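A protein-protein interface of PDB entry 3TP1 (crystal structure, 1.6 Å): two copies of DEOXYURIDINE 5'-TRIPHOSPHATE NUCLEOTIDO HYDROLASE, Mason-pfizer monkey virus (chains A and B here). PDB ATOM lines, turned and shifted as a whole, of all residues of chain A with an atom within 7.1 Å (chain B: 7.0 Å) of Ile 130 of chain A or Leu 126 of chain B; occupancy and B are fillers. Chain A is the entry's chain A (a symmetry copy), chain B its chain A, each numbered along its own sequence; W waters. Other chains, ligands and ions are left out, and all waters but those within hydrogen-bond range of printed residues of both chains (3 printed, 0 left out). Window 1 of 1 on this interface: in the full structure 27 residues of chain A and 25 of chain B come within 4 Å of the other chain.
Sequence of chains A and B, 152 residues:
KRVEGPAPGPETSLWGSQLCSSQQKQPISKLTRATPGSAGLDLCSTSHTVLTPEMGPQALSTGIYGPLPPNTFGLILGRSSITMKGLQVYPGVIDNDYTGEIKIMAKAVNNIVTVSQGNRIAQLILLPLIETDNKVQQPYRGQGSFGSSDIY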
ATOM      1  N   ASN A  71      -3.224  -9.199  -0.223  1.00  0.00           N
ATOM      2  CA  ASN A  71      -3.848 -10.508  -0.349  1.00  0.00           C
ATOM      3  C   ASN A  71      -4.725 -10.645  -1.574  1.00  0.00           C
ATOM      4  O   ASN A  71      -5.602 -11.518  -1.605  1.00  0.00           O
ATOM      5  CB  ASN A  71      -4.661 -10.826   0.907  1.00  0.00           C
ATOM      6  CG  ASN A  71      -3.813 -10.694   2.197  1.00  0.00           C
ATOM      7  OD1 ASN A  71      -2.748 -11.298   2.302  1.00  0.00           O
ATOM      8  ND2 ASN A  71      -4.292  -9.895   3.153  1.00  0.00           N
ATOM      9  N   PHE A  73      -4.799 -10.520  -6.125  1.00  0.00           N
ATOM     10  CA  PHE A  73      -4.101 -10.328  -7.387  1.00  0.00           C
ATOM     11  C   PHE A  73      -5.139  -9.866  -8.390  1.00  0.00           C
ATOM     12  O   PHE A  73      -6.341  -9.808  -8.076  1.00  0.00           O
ATOM     13  CB  PHE A  73      -3.345 -11.580  -7.826  1.00  0.00           C
ATOM     14  CG  PHE A  73      -4.249 -12.685  -8.370  1.00  0.00           C
ATOM     15  CD1 PHE A  73      -4.436 -12.857  -9.763  1.00  0.00           C
ATOM     16  CD2 PHE A  73      -4.975 -13.504  -7.509  1.00  0.00           C
ATOM     17  CE1 PHE A  73      -5.274 -13.850 -10.255  1.00  0.00           C
ATOM     18  CE2 PHE A  73      -5.813 -14.534  -8.020  1.00  0.00           C
ATOM     19  CZ  PHE A  73      -5.956 -14.679  -9.381  1.00  0.00           C
ATOM     20  N   LEU A 127      -9.064 -10.742  -7.207  1.00  0.00           N
ATOM     21  CA  LEU A 127      -9.344 -12.066  -6.701  1.00  0.00           C
ATOM     22  C   LEU A 127      -8.398 -12.331  -5.521  1.00  0.00           C
ATOM     23  O   LEU A 127      -7.326 -11.732  -5.422  1.00  0.00           O
ATOM     24  CB  LEU A 127      -9.033 -13.049  -7.779  1.00  0.00           C
ATOM     25  CG  LEU A 127     -10.067 -13.037  -8.936  1.00  0.00           C
ATOM     26  CD1 LEU A 127      -9.622 -13.899 -10.100  1.00  0.00           C
ATOM     27  CD2 LEU A 127     -11.462 -13.454  -8.425  1.00  0.00           C
ATOM     28  N   PRO A 128      -8.802 -13.238  -4.627  1.00  0.00           N
ATOM     29  CA  PRO A 128      -7.974 -13.577  -3.477  1.00  0.00           C
ATOM     30  C   PRO A 128      -6.696 -14.286  -3.924  1.00  0.00           C
ATOM     31  O   PRO A 128      -6.707 -15.111  -4.859  1.00  0.00           O
ATOM     32  CB  PRO A 128      -8.864 -14.521  -2.672  1.00  0.00           C
ATOM     33  CG  PRO A 128      -9.822 -15.090  -3.649  1.00  0.00           C
ATOM     34  CD  PRO A 128     -10.037 -14.040  -4.710  1.00  0.00           C
ATOM     35  N   LEU A 129      -5.592 -13.917  -3.281  1.00  0.00           N
ATOM     36  CA  LEU A 129      -4.320 -14.572  -3.555  1.00  0.00           C
ATOM     37  C   LEU A 129      -4.138 -15.640  -2.518  1.00  0.00           C
ATOM     38  O   LEU A 129      -3.973 -15.352  -1.339  1.00  0.00           O
ATOM     39  CB  LEU A 129      -3.212 -13.517  -3.488  1.00  0.00           C
ATOM     40  CG  LEU A 129      -1.767 -13.948  -3.684  1.00  0.00           C
ATOM     41  CD1 LEU A 129      -1.501 -14.745  -4.964  1.00  0.00           C
ATOM     42  CD2 LEU A 129      -0.909 -12.669  -3.681  1.00  0.00           C
ATOM     43  N   ILE A 130      -4.187 -16.894  -2.968  1.00  0.00           N
ATOM     44  CA  ILE A 130      -4.029 -18.003  -2.058  1.00  0.00           C
ATOM     45  C   ILE A 130      -2.553 -18.246  -1.829  1.00  0.00           C
ATOM     46  O   ILE A 130      -1.790 -18.277  -2.773  1.00  0.00           O
ATOM     47  CB  ILE A 130      -4.703 -19.260  -2.644  1.00  0.00           C
ATOM     48  CG1 ILE A 130      -6.223 -19.091  -2.569  1.00  0.00           C
ATOM     49  CG2 ILE A 130      -4.245 -20.529  -1.945  1.00  0.00           C
ATOM     50  CD1 ILE A 130      -6.968 -20.078  -3.386  1.00  0.00           C
ATOM     51  N   GLU A 131      -2.186 -18.469  -0.563  1.00  0.00           N
ATOM     52  CA  GLU A 131      -0.815 -18.760  -0.191  1.00  0.00           C
ATOM     53  C   GLU A 131      -0.597 -20.273  -0.290  1.00  0.00           C
ATOM     54  O   GLU A 131      -1.506 -21.071  -0.050  1.00  0.00           O
ATOM     55  CB  GLU A 131      -0.544 -18.235   1.235  1.00  0.00           C
ATOM     56  CG  GLU A 131      -0.614 -16.693   1.350  1.00  0.00           C
ATOM     57  CD  GLU A 131       0.146 -16.145   2.561  1.00  0.00           C
ATOM     58  N   THR A 132       0.595 -20.668  -0.723  1.00  0.00           N
ATOM     59  CA  THR A 132       0.936 -22.066  -0.820  1.00  0.00           C
ATOM     60  C   THR A 132       2.402 -22.179  -0.406  1.00  0.00           C
ATOM     61  O   THR A 132       3.107 -21.149  -0.310  1.00  0.00           O
ATOM     62  CB  THR A 132       0.795 -22.597  -2.272  1.00  0.00           C
ATOM     63  OG1 THR A 132       1.870 -22.094  -3.074  1.00  0.00           O
ATOM     64  CG2 THR A 132      -0.543 -22.198  -2.904  1.00  0.00           C
ATOM     65  N   ASN A 134       4.665 -23.524  -2.264  1.00  0.00           N
ATOM     66  CA  ASN A 134       5.513 -23.637  -3.438  1.00  0.00           C
ATOM     67  C   ASN A 134       6.730 -22.760  -3.295  1.00  0.00           C
ATOM     68  O   ASN A 134       6.639 -21.629  -2.836  1.00  0.00           O
ATOM     69  CB  ASN A 134       4.776 -23.250  -4.714  1.00  0.00           C
ATOM     70  CG  ASN A 134       3.721 -24.257  -5.084  1.00  0.00           C
ATOM     71  OD1 ASN A 134       3.962 -25.173  -5.893  1.00  0.00           O
ATOM     72  ND2 ASN A 134       2.533 -24.100  -4.493  1.00  0.00           N
ATOM     73  N   ILE B  28       1.602 -30.645  -8.238  1.00  0.00           N
ATOM     74  CA  ILE B  28       1.745 -29.210  -8.367  1.00  0.00           C
ATOM     75  C   ILE B  28       2.630 -28.581  -7.288  1.00  0.00           C
ATOM     76  O   ILE B  28       3.068 -27.441  -7.448  1.00  0.00           O
ATOM     77  CB  ILE B  28       0.372 -28.453  -8.483  1.00  0.00           C
ATOM     78  CG1 ILE B  28      -0.385 -28.549  -7.206  1.00  0.00           C
ATOM     79  CG2 ILE B  28      -0.469 -28.989  -9.658  1.00  0.00           C
ATOM     80  CD1 ILE B  28      -0.934 -27.223  -6.838  1.00  0.00           C
ATOM     81  N   ARG B  33       7.158 -20.237  -8.026  1.00  0.00           N
ATOM     82  CA  ARG B  33       6.675 -18.897  -8.325  1.00  0.00           C
ATOM     83  C   ARG B  33       7.861 -18.101  -8.744  1.00  0.00           C
ATOM     84  O   ARG B  33       8.962 -18.356  -8.236  1.00  0.00           O
ATOM     85  CB  ARG B  33       6.172 -18.239  -7.051  1.00  0.00           C
ATOM     86  CG  ARG B  33       4.788 -18.597  -6.733  1.00  0.00           C
ATOM     87  CD  ARG B  33       4.266 -17.879  -5.480  1.00  0.00           C
ATOM     88  NE  ARG B  33       3.266 -18.788  -4.952  1.00  0.00           N
ATOM     89  CZ  ARG B  33       2.028 -18.956  -5.423  1.00  0.00           C
ATOM     90  NH1 ARG B  33       1.536 -18.179  -6.386  1.00  0.00           N
ATOM     91  NH2 ARG B  33       1.252 -19.882  -4.888  1.00  0.00           N
ATOM     92  N   SER B  38       4.099 -13.203  -6.920  1.00  0.00           N
ATOM     93  CA  SER B  38       3.530 -13.759  -8.177  1.00  0.00           C
ATOM     94  C   SER B  38       2.244 -14.526  -7.904  1.00  0.00           C
ATOM     95  O   SER B  38       2.210 -15.392  -7.046  1.00  0.00           O
ATOM     96  CB  SER B  38       4.535 -14.671  -8.890  1.00  0.00           C
ATOM     97  OG  SER B  38       5.677 -13.956  -9.340  1.00  0.00           O
ATOM     98  N   ALA B  39       1.173 -14.213  -8.642  1.00  0.00           N
ATOM     99  CA  ALA B  39      -0.078 -14.927  -8.510  1.00  0.00           C
ATOM    100  C   ALA B  39       0.067 -16.349  -9.048  1.00  0.00           C
ATOM    101  O   ALA B  39      -0.551 -17.271  -8.536  1.00  0.00           O
ATOM    102  CB  ALA B  39      -1.143 -14.188  -9.251  1.00  0.00           C
ATOM    103  N   GLY B  40       0.869 -16.538 -10.081  1.00  0.00           N
ATOM    104  CA  GLY B  40       0.822 -17.837 -10.769  1.00  0.00           C
ATOM    105  C   GLY B  40       2.009 -18.719 -10.489  1.00  0.00           C
ATOM    106  O   GLY B  40       3.114 -18.229 -10.146  1.00  0.00           O
ATOM    107  N   LEU B  41       1.761 -20.024 -10.605  1.00  0.00           N
ATOM    108  CA  LEU B  41       2.853 -21.007 -10.560  1.00  0.00           C
ATOM    109  C   LEU B  41       3.256 -21.310 -11.976  1.00  0.00           C
ATOM    110  O   LEU B  41       2.422 -21.628 -12.802  1.00  0.00           O
ATOM    111  CB  LEU B  41       2.333 -22.275  -9.896  1.00  0.00           C
ATOM    112  CG  LEU B  41       1.919 -22.119  -8.425  1.00  0.00           C
ATOM    113  CD1 LEU B  41       1.122 -23.357  -7.907  1.00  0.00           C
ATOM    114  CD2 LEU B  41       3.139 -21.842  -7.577  1.00  0.00           C
ATOM    115  N   LEU B  68      -5.505 -30.732  -6.851  1.00  0.00           N
ATOM    116  CA  LEU B  68      -5.205 -29.448  -6.299  1.00  0.00           C
ATOM    117  C   LEU B  68      -5.500 -29.457  -4.801  1.00  0.00           C
ATOM    118  O   LEU B  68      -6.096 -30.415  -4.284  1.00  0.00           O
ATOM    119  CB  LEU B  68      -6.099 -28.435  -6.964  1.00  0.00           C
ATOM    120  CG  LEU B  68      -5.925 -28.327  -8.486  1.00  0.00           C
ATOM    121  CD1 LEU B  68      -6.516 -27.034  -8.863  1.00  0.00           C
ATOM    122  CD2 LEU B  68      -4.519 -28.350  -8.917  1.00  0.00           C
ATOM    123  N   PRO B  69      -4.981 -28.460  -4.077  1.00  0.00           N
ATOM    124  CA  PRO B  69      -5.233 -28.388  -2.644  1.00  0.00           C
ATOM    125  C   PRO B  69      -6.721 -28.347  -2.321  1.00  0.00           C
ATOM    126  O   PRO B  69      -7.520 -27.848  -3.123  1.00  0.00           O
ATOM    127  CB  PRO B  69      -4.568 -27.060  -2.245  1.00  0.00           C
ATOM    128  CG  PRO B  69      -3.478 -26.859  -3.241  1.00  0.00           C
ATOM    129  CD  PRO B  69      -4.043 -27.401  -4.529  1.00  0.00           C
ATOM    130  N   ASN B  71     -10.432 -27.472  -1.481  1.00  0.00           N
ATOM    131  CA  ASN B  71     -11.239 -26.267  -1.602  1.00  0.00           C
ATOM    132  C   ASN B  71     -10.700 -25.277  -2.610  1.00  0.00           C
ATOM    133  O   ASN B  71     -11.033 -24.087  -2.538  1.00  0.00           O
ATOM    134  CB  ASN B  71     -11.382 -25.591  -0.238  1.00  0.00           C
ATOM    135  CG  ASN B  71     -11.926 -26.563   0.839  1.00  0.00           C
ATOM    136  OD1 ASN B  71     -12.966 -27.186   0.642  1.00  0.00           O
ATOM    137  ND2 ASN B  71     -11.205 -26.688   1.956  1.00  0.00           N
ATOM    138  N   THR B  72      -9.846 -25.756  -3.522  1.00  0.00           N
ATOM    139  CA  THR B  72      -9.342 -24.861  -4.596  1.00  0.00           C
ATOM    140  C   THR B  72      -9.586 -25.474  -5.964  1.00  0.00           C
ATOM    141  O   THR B  72      -9.674 -26.722  -6.093  1.00  0.00           O
ATOM    142  CB  THR B  72      -7.803 -24.549  -4.445  1.00  0.00           C
ATOM    143  OG1 THR B  72      -7.031 -25.658  -4.891  1.00  0.00           O
ATOM    144  CG2 THR B  72      -7.417 -24.211  -2.988  1.00  0.00           C
ATOM    145  N   PHE B  73      -9.646 -24.634  -6.993  1.00  0.00           N
ATOM    146  CA  PHE B  73      -9.555 -25.150  -8.350  1.00  0.00           C
ATOM    147  C   PHE B  73      -8.471 -24.352  -9.045  1.00  0.00           C
ATOM    148  O   PHE B  73      -7.919 -23.398  -8.469  1.00  0.00           O
ATOM    149  CB  PHE B  73     -10.900 -25.108  -9.075  1.00  0.00           C
ATOM    150  CG  PHE B  73     -11.316 -23.707  -9.519  1.00  0.00           C
ATOM    151  CD1 PHE B  73     -11.098 -23.264 -10.846  1.00  0.00           C
ATOM    152  CD2 PHE B  73     -11.853 -22.798  -8.610  1.00  0.00           C
ATOM    153  CE1 PHE B  73     -11.459 -21.982 -11.242  1.00  0.00           C
ATOM    154  CE2 PHE B  73     -12.242 -21.495  -9.027  1.00  0.00           C
ATOM    155  CZ  PHE B  73     -12.026 -21.108 -10.330  1.00  0.00           C
ATOM    156  N   GLY B  74      -8.128 -24.715 -10.280  1.00  0.00           N
ATOM    157  CA  GLY B  74      -7.008 -23.985 -10.929  1.00  0.00           C
ATOM    158  C   GLY B  74      -7.465 -23.300 -12.219  1.00  0.00           C
ATOM    159  O   GLY B  74      -8.429 -23.725 -12.861  1.00  0.00           O
ATOM    160  N   LEU B  75      -6.772 -22.211 -12.576  1.00  0.00           N
ATOM    161  CA  LEU B  75      -6.938 -21.614 -13.903  1.00  0.00           C
ATOM    162  C   LEU B  75      -5.576 -21.555 -14.535  1.00  0.00           C
ATOM    163  O   LEU B  75      -4.665 -21.045 -13.908  1.00  0.00           O
ATOM    164  CB  LEU B  75      -7.430 -20.182 -13.787  1.00  0.00           C
ATOM    165  CG  LEU B  75      -8.888 -19.730 -13.733  1.00  0.00           C
ATOM    166  CD1 LEU B  75      -8.931 -18.223 -14.131  1.00  0.00           C
ATOM    167  CD2 LEU B  75      -9.864 -20.573 -14.653  1.00  0.00           C
ATOM    168  N   LEU B 124      -0.212 -21.399 -13.573  1.00  0.00           N
ATOM    169  CA  LEU B 124      -1.338 -21.921 -12.869  1.00  0.00           C
ATOM    170  C   LEU B 124      -1.708 -20.973 -11.757  1.00  0.00           C
ATOM    171  O   LEU B 124      -0.916 -20.761 -10.843  1.00  0.00           O
ATOM    172  CB  LEU B 124      -0.971 -23.287 -12.250  1.00  0.00           C
ATOM    173  CG  LEU B 124      -2.077 -23.992 -11.436  1.00  0.00           C
ATOM    174  CD1 LEU B 124      -3.279 -24.369 -12.332  1.00  0.00           C
ATOM    175  CD2 LEU B 124      -1.489 -25.222 -10.764  1.00  0.00           C
ATOM    176  N   ILE B 125      -2.952 -20.499 -11.779  1.00  0.00           N
ATOM    177  CA  ILE B 125      -3.480 -19.721 -10.658  1.00  0.00           C
ATOM    178  C   ILE B 125      -4.461 -20.555  -9.842  1.00  0.00           C
ATOM    179  O   ILE B 125      -5.279 -21.242 -10.406  1.00  0.00           O
ATOM    180  CB  ILE B 125      -4.149 -18.468 -11.225  1.00  0.00           C
ATOM    181  CG1 ILE B 125      -3.077 -17.470 -11.718  1.00  0.00           C
ATOM    182  CG2 ILE B 125      -5.096 -17.842 -10.205  1.00  0.00           C
ATOM    183  CD1 ILE B 125      -3.368 -16.998 -13.053  1.00  0.00           C
ATOM    184  N   LEU B 126      -4.344 -20.531  -8.518  1.00  0.00           N
ATOM    185  CA  LEU B 126      -5.293 -21.261  -7.629  1.00  0.00           C
ATOM    186  C   LEU B 126      -6.355 -20.285  -7.113  1.00  0.00           C
ATOM    187  O   LEU B 126      -6.030 -19.148  -6.705  1.00  0.00           O
ATOM    188  CB  LEU B 126      -4.540 -21.850  -6.444  1.00  0.00           C
ATOM    189  CG  LEU B 126      -3.443 -22.778  -6.890  1.00  0.00           C
ATOM    190  CD1 LEU B 126      -2.707 -23.034  -5.598  1.00  0.00           C
ATOM    191  CD2 LEU B 126      -4.055 -24.112  -7.422  1.00  0.00           C
ATOM    192  N   LEU B 127      -7.617 -20.727  -7.122  1.00  0.00           N
ATOM    193  CA  LEU B 127      -8.724 -19.896  -6.708  1.00  0.00           C
ATOM    194  C   LEU B 127      -9.633 -20.739  -5.801  1.00  0.00           C
ATOM    195  O   LEU B 127      -9.642 -21.968  -5.880  1.00  0.00           O
ATOM    196  CB  LEU B 127      -9.500 -19.519  -7.925  1.00  0.00           C
ATOM    197  CG  LEU B 127      -8.773 -18.478  -8.817  1.00  0.00           C
ATOM    198  CD1 LEU B 127      -9.490 -18.264 -10.135  1.00  0.00           C
ATOM    199  CD2 LEU B 127      -8.578 -17.150  -8.057  1.00  0.00           C
ATOM    200  N   PRO B 128     -10.403 -20.066  -4.940  1.00  0.00           N
ATOM    201  CA  PRO B 128     -11.314 -20.766  -4.044  1.00  0.00           C
ATOM    202  C   PRO B 128     -12.435 -21.441  -4.834  1.00  0.00           C
ATOM    203  O   PRO B 128     -12.951 -20.888  -5.825  1.00  0.00           O
ATOM    204  CB  PRO B 128     -11.868 -19.648  -3.166  1.00  0.00           C
ATOM    205  CG  PRO B 128     -11.712 -18.407  -3.961  1.00  0.00           C
ATOM    206  CD  PRO B 128     -10.495 -18.598  -4.831  1.00  0.00           C
ATOM    207  N   LEU B 129     -12.764 -22.660  -4.416  1.00  0.00           N
ATOM    208  CA  LEU B 129     -13.870 -23.381  -5.032  1.00  0.00           C
ATOM    209  C   LEU B 129     -15.081 -23.149  -4.180  1.00  0.00           C
ATOM    210  O   LEU B 129     -15.147 -23.599  -3.042  1.00  0.00           O
ATOM    211  CB  LEU B 129     -13.497 -24.865  -5.102  1.00  0.00           C
ATOM    212  CG  LEU B 129     -14.507 -25.856  -5.657  1.00  0.00           C
ATOM    213  CD1 LEU B 129     -15.061 -25.505  -7.041  1.00  0.00           C
ATOM    214  CD2 LEU B 129     -13.811 -27.230  -5.710  1.00  0.00           C
HETATM  215  O   HOH W   1      -4.874 -17.070  -5.753  1.00  0.00           O
HETATM  216  O   HOH W   2       4.516 -19.895  -2.800  1.00  0.00           O
HETATM  217  O   HOH W   3      -1.504 -19.376  -5.199  1.00  0.00           O
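Water W1 lies within hydrogen-bond range of the backbone carbonyl oxygen (O) of Leu 126 of chain B (2.6 Å), the backbone carbonyl oxygen (O) of Pro 128 of chain A (2.8 Å) and the backbone NH (N) of Ile 130 of chain A (2.9 Å). Water W3 lies within hydrogen-bond range of O of Ile 130 of chain A (2.7 Å) and NH2 of Arg 33 of chain B (2.8 Å). Water W2 lies within hydrogen-bond range of NE of Arg 33 of chain B (2.7 Å), O of Asn 134 of chain A (2.7 Å) and O of Thr 132 of chain A (3.1 Å).
Phe 73 of chain A touches Leu 127 of chain B, but with the chains exchanged Leu 127 of chain A does not touch Phe 73 of chain B (7.6 Å). Leu 127 of chain A touches its own counterpart, Leu 127 of chain B. Pro 128 of chain B touches its own counterpart, Pro 128 of chain A. 5 positions are printed for both chains.
Ile 130 of chain A touches three residues of chain B. Of the printed residues of chain B, Asn 134 of chain A touches Ile 28 and Leu 41. Of the printed residues of chain A, Ala 39 of chain B touches Phe 73 and Leu 129. Of the printed residues of chain A, Leu 126 of chain B touches Ile 130 and Thr 132. Leu 129 of chain B touches none of the printed residues of chain A. The nearest residue of chain B that does not touch Ile 130 of chain A is Arg 33 of chain B (4.04 Å).
Printed residues of chain B that touch a printed residue of chain A: Ile 28, Arg 33, Ala 39, Leu 41, Ile 125, Leu 126, Leu 127 and Pro 128. Among the printed residues, 13 pairs touch across the chains. Among the printed residues, no Asp or Glu carboxylate lies within 4 Å of a Lys or Arg side-chain nitrogen of the other chain.
OD1 of Asn 134 of chain A lies close to O of Ile 28 of chain B, at 2.9 Å. NH2 of Arg 33 of chain B lies within hydrogen-bond range of OG1 of Thr 132 of chain A, at 2.9 Å.
Among the printed residues, pairs that only touch across the chains: Phe 73 of chain A with Ile 125 of chain B, Asn 134 of chain A with Leu 41 of chain B, Thr 132 of chain A with Leu 126 of chain B, Phe 73 of chain A with Ala 39 of chain B, Ile 130 of chain A with Leu 126 of chain B, Ile 130 of chain A with Leu 127 of chain B, Pro 128 of chain A with Pro 128 of chain B, Ile 130 of chain A with Pro 128 of chain B, Phe 73 of chain A with Leu 127 of chain B, Leu 129 of chain A with Ala 39 of chain B and Leu 127 of chain A with Leu 127 of chain B.
The guanidinium group (NH1) of Arg 33 of chain B sits at hydrogen-bond distance from the backbone carbonyl oxygen (O) of Ser 38 of chain B (2.9 Å). O of Leu 127 of chain B sits at hydrogen-bond distance from N of Phe 73 of chain B (2.9 Å). N of Ile 125 of chain B is in hydrogen-bond range of O of Leu 75 of chain B (2.8 Å). O of Asn 71 of chain A sits at hydrogen-bond distance from N of Leu 129 of chain A (2.9 Å). The backbone NH of Phe 73 of chain A sits at hydrogen-bond distance from the backbone carbonyl oxygen of Leu 127 of chain A, at 2.9 Å. OG1 of Thr 132 of chain A lies within hydrogen-bond range of ND2 of Asn 134 of chain A, 2.5 Å away.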
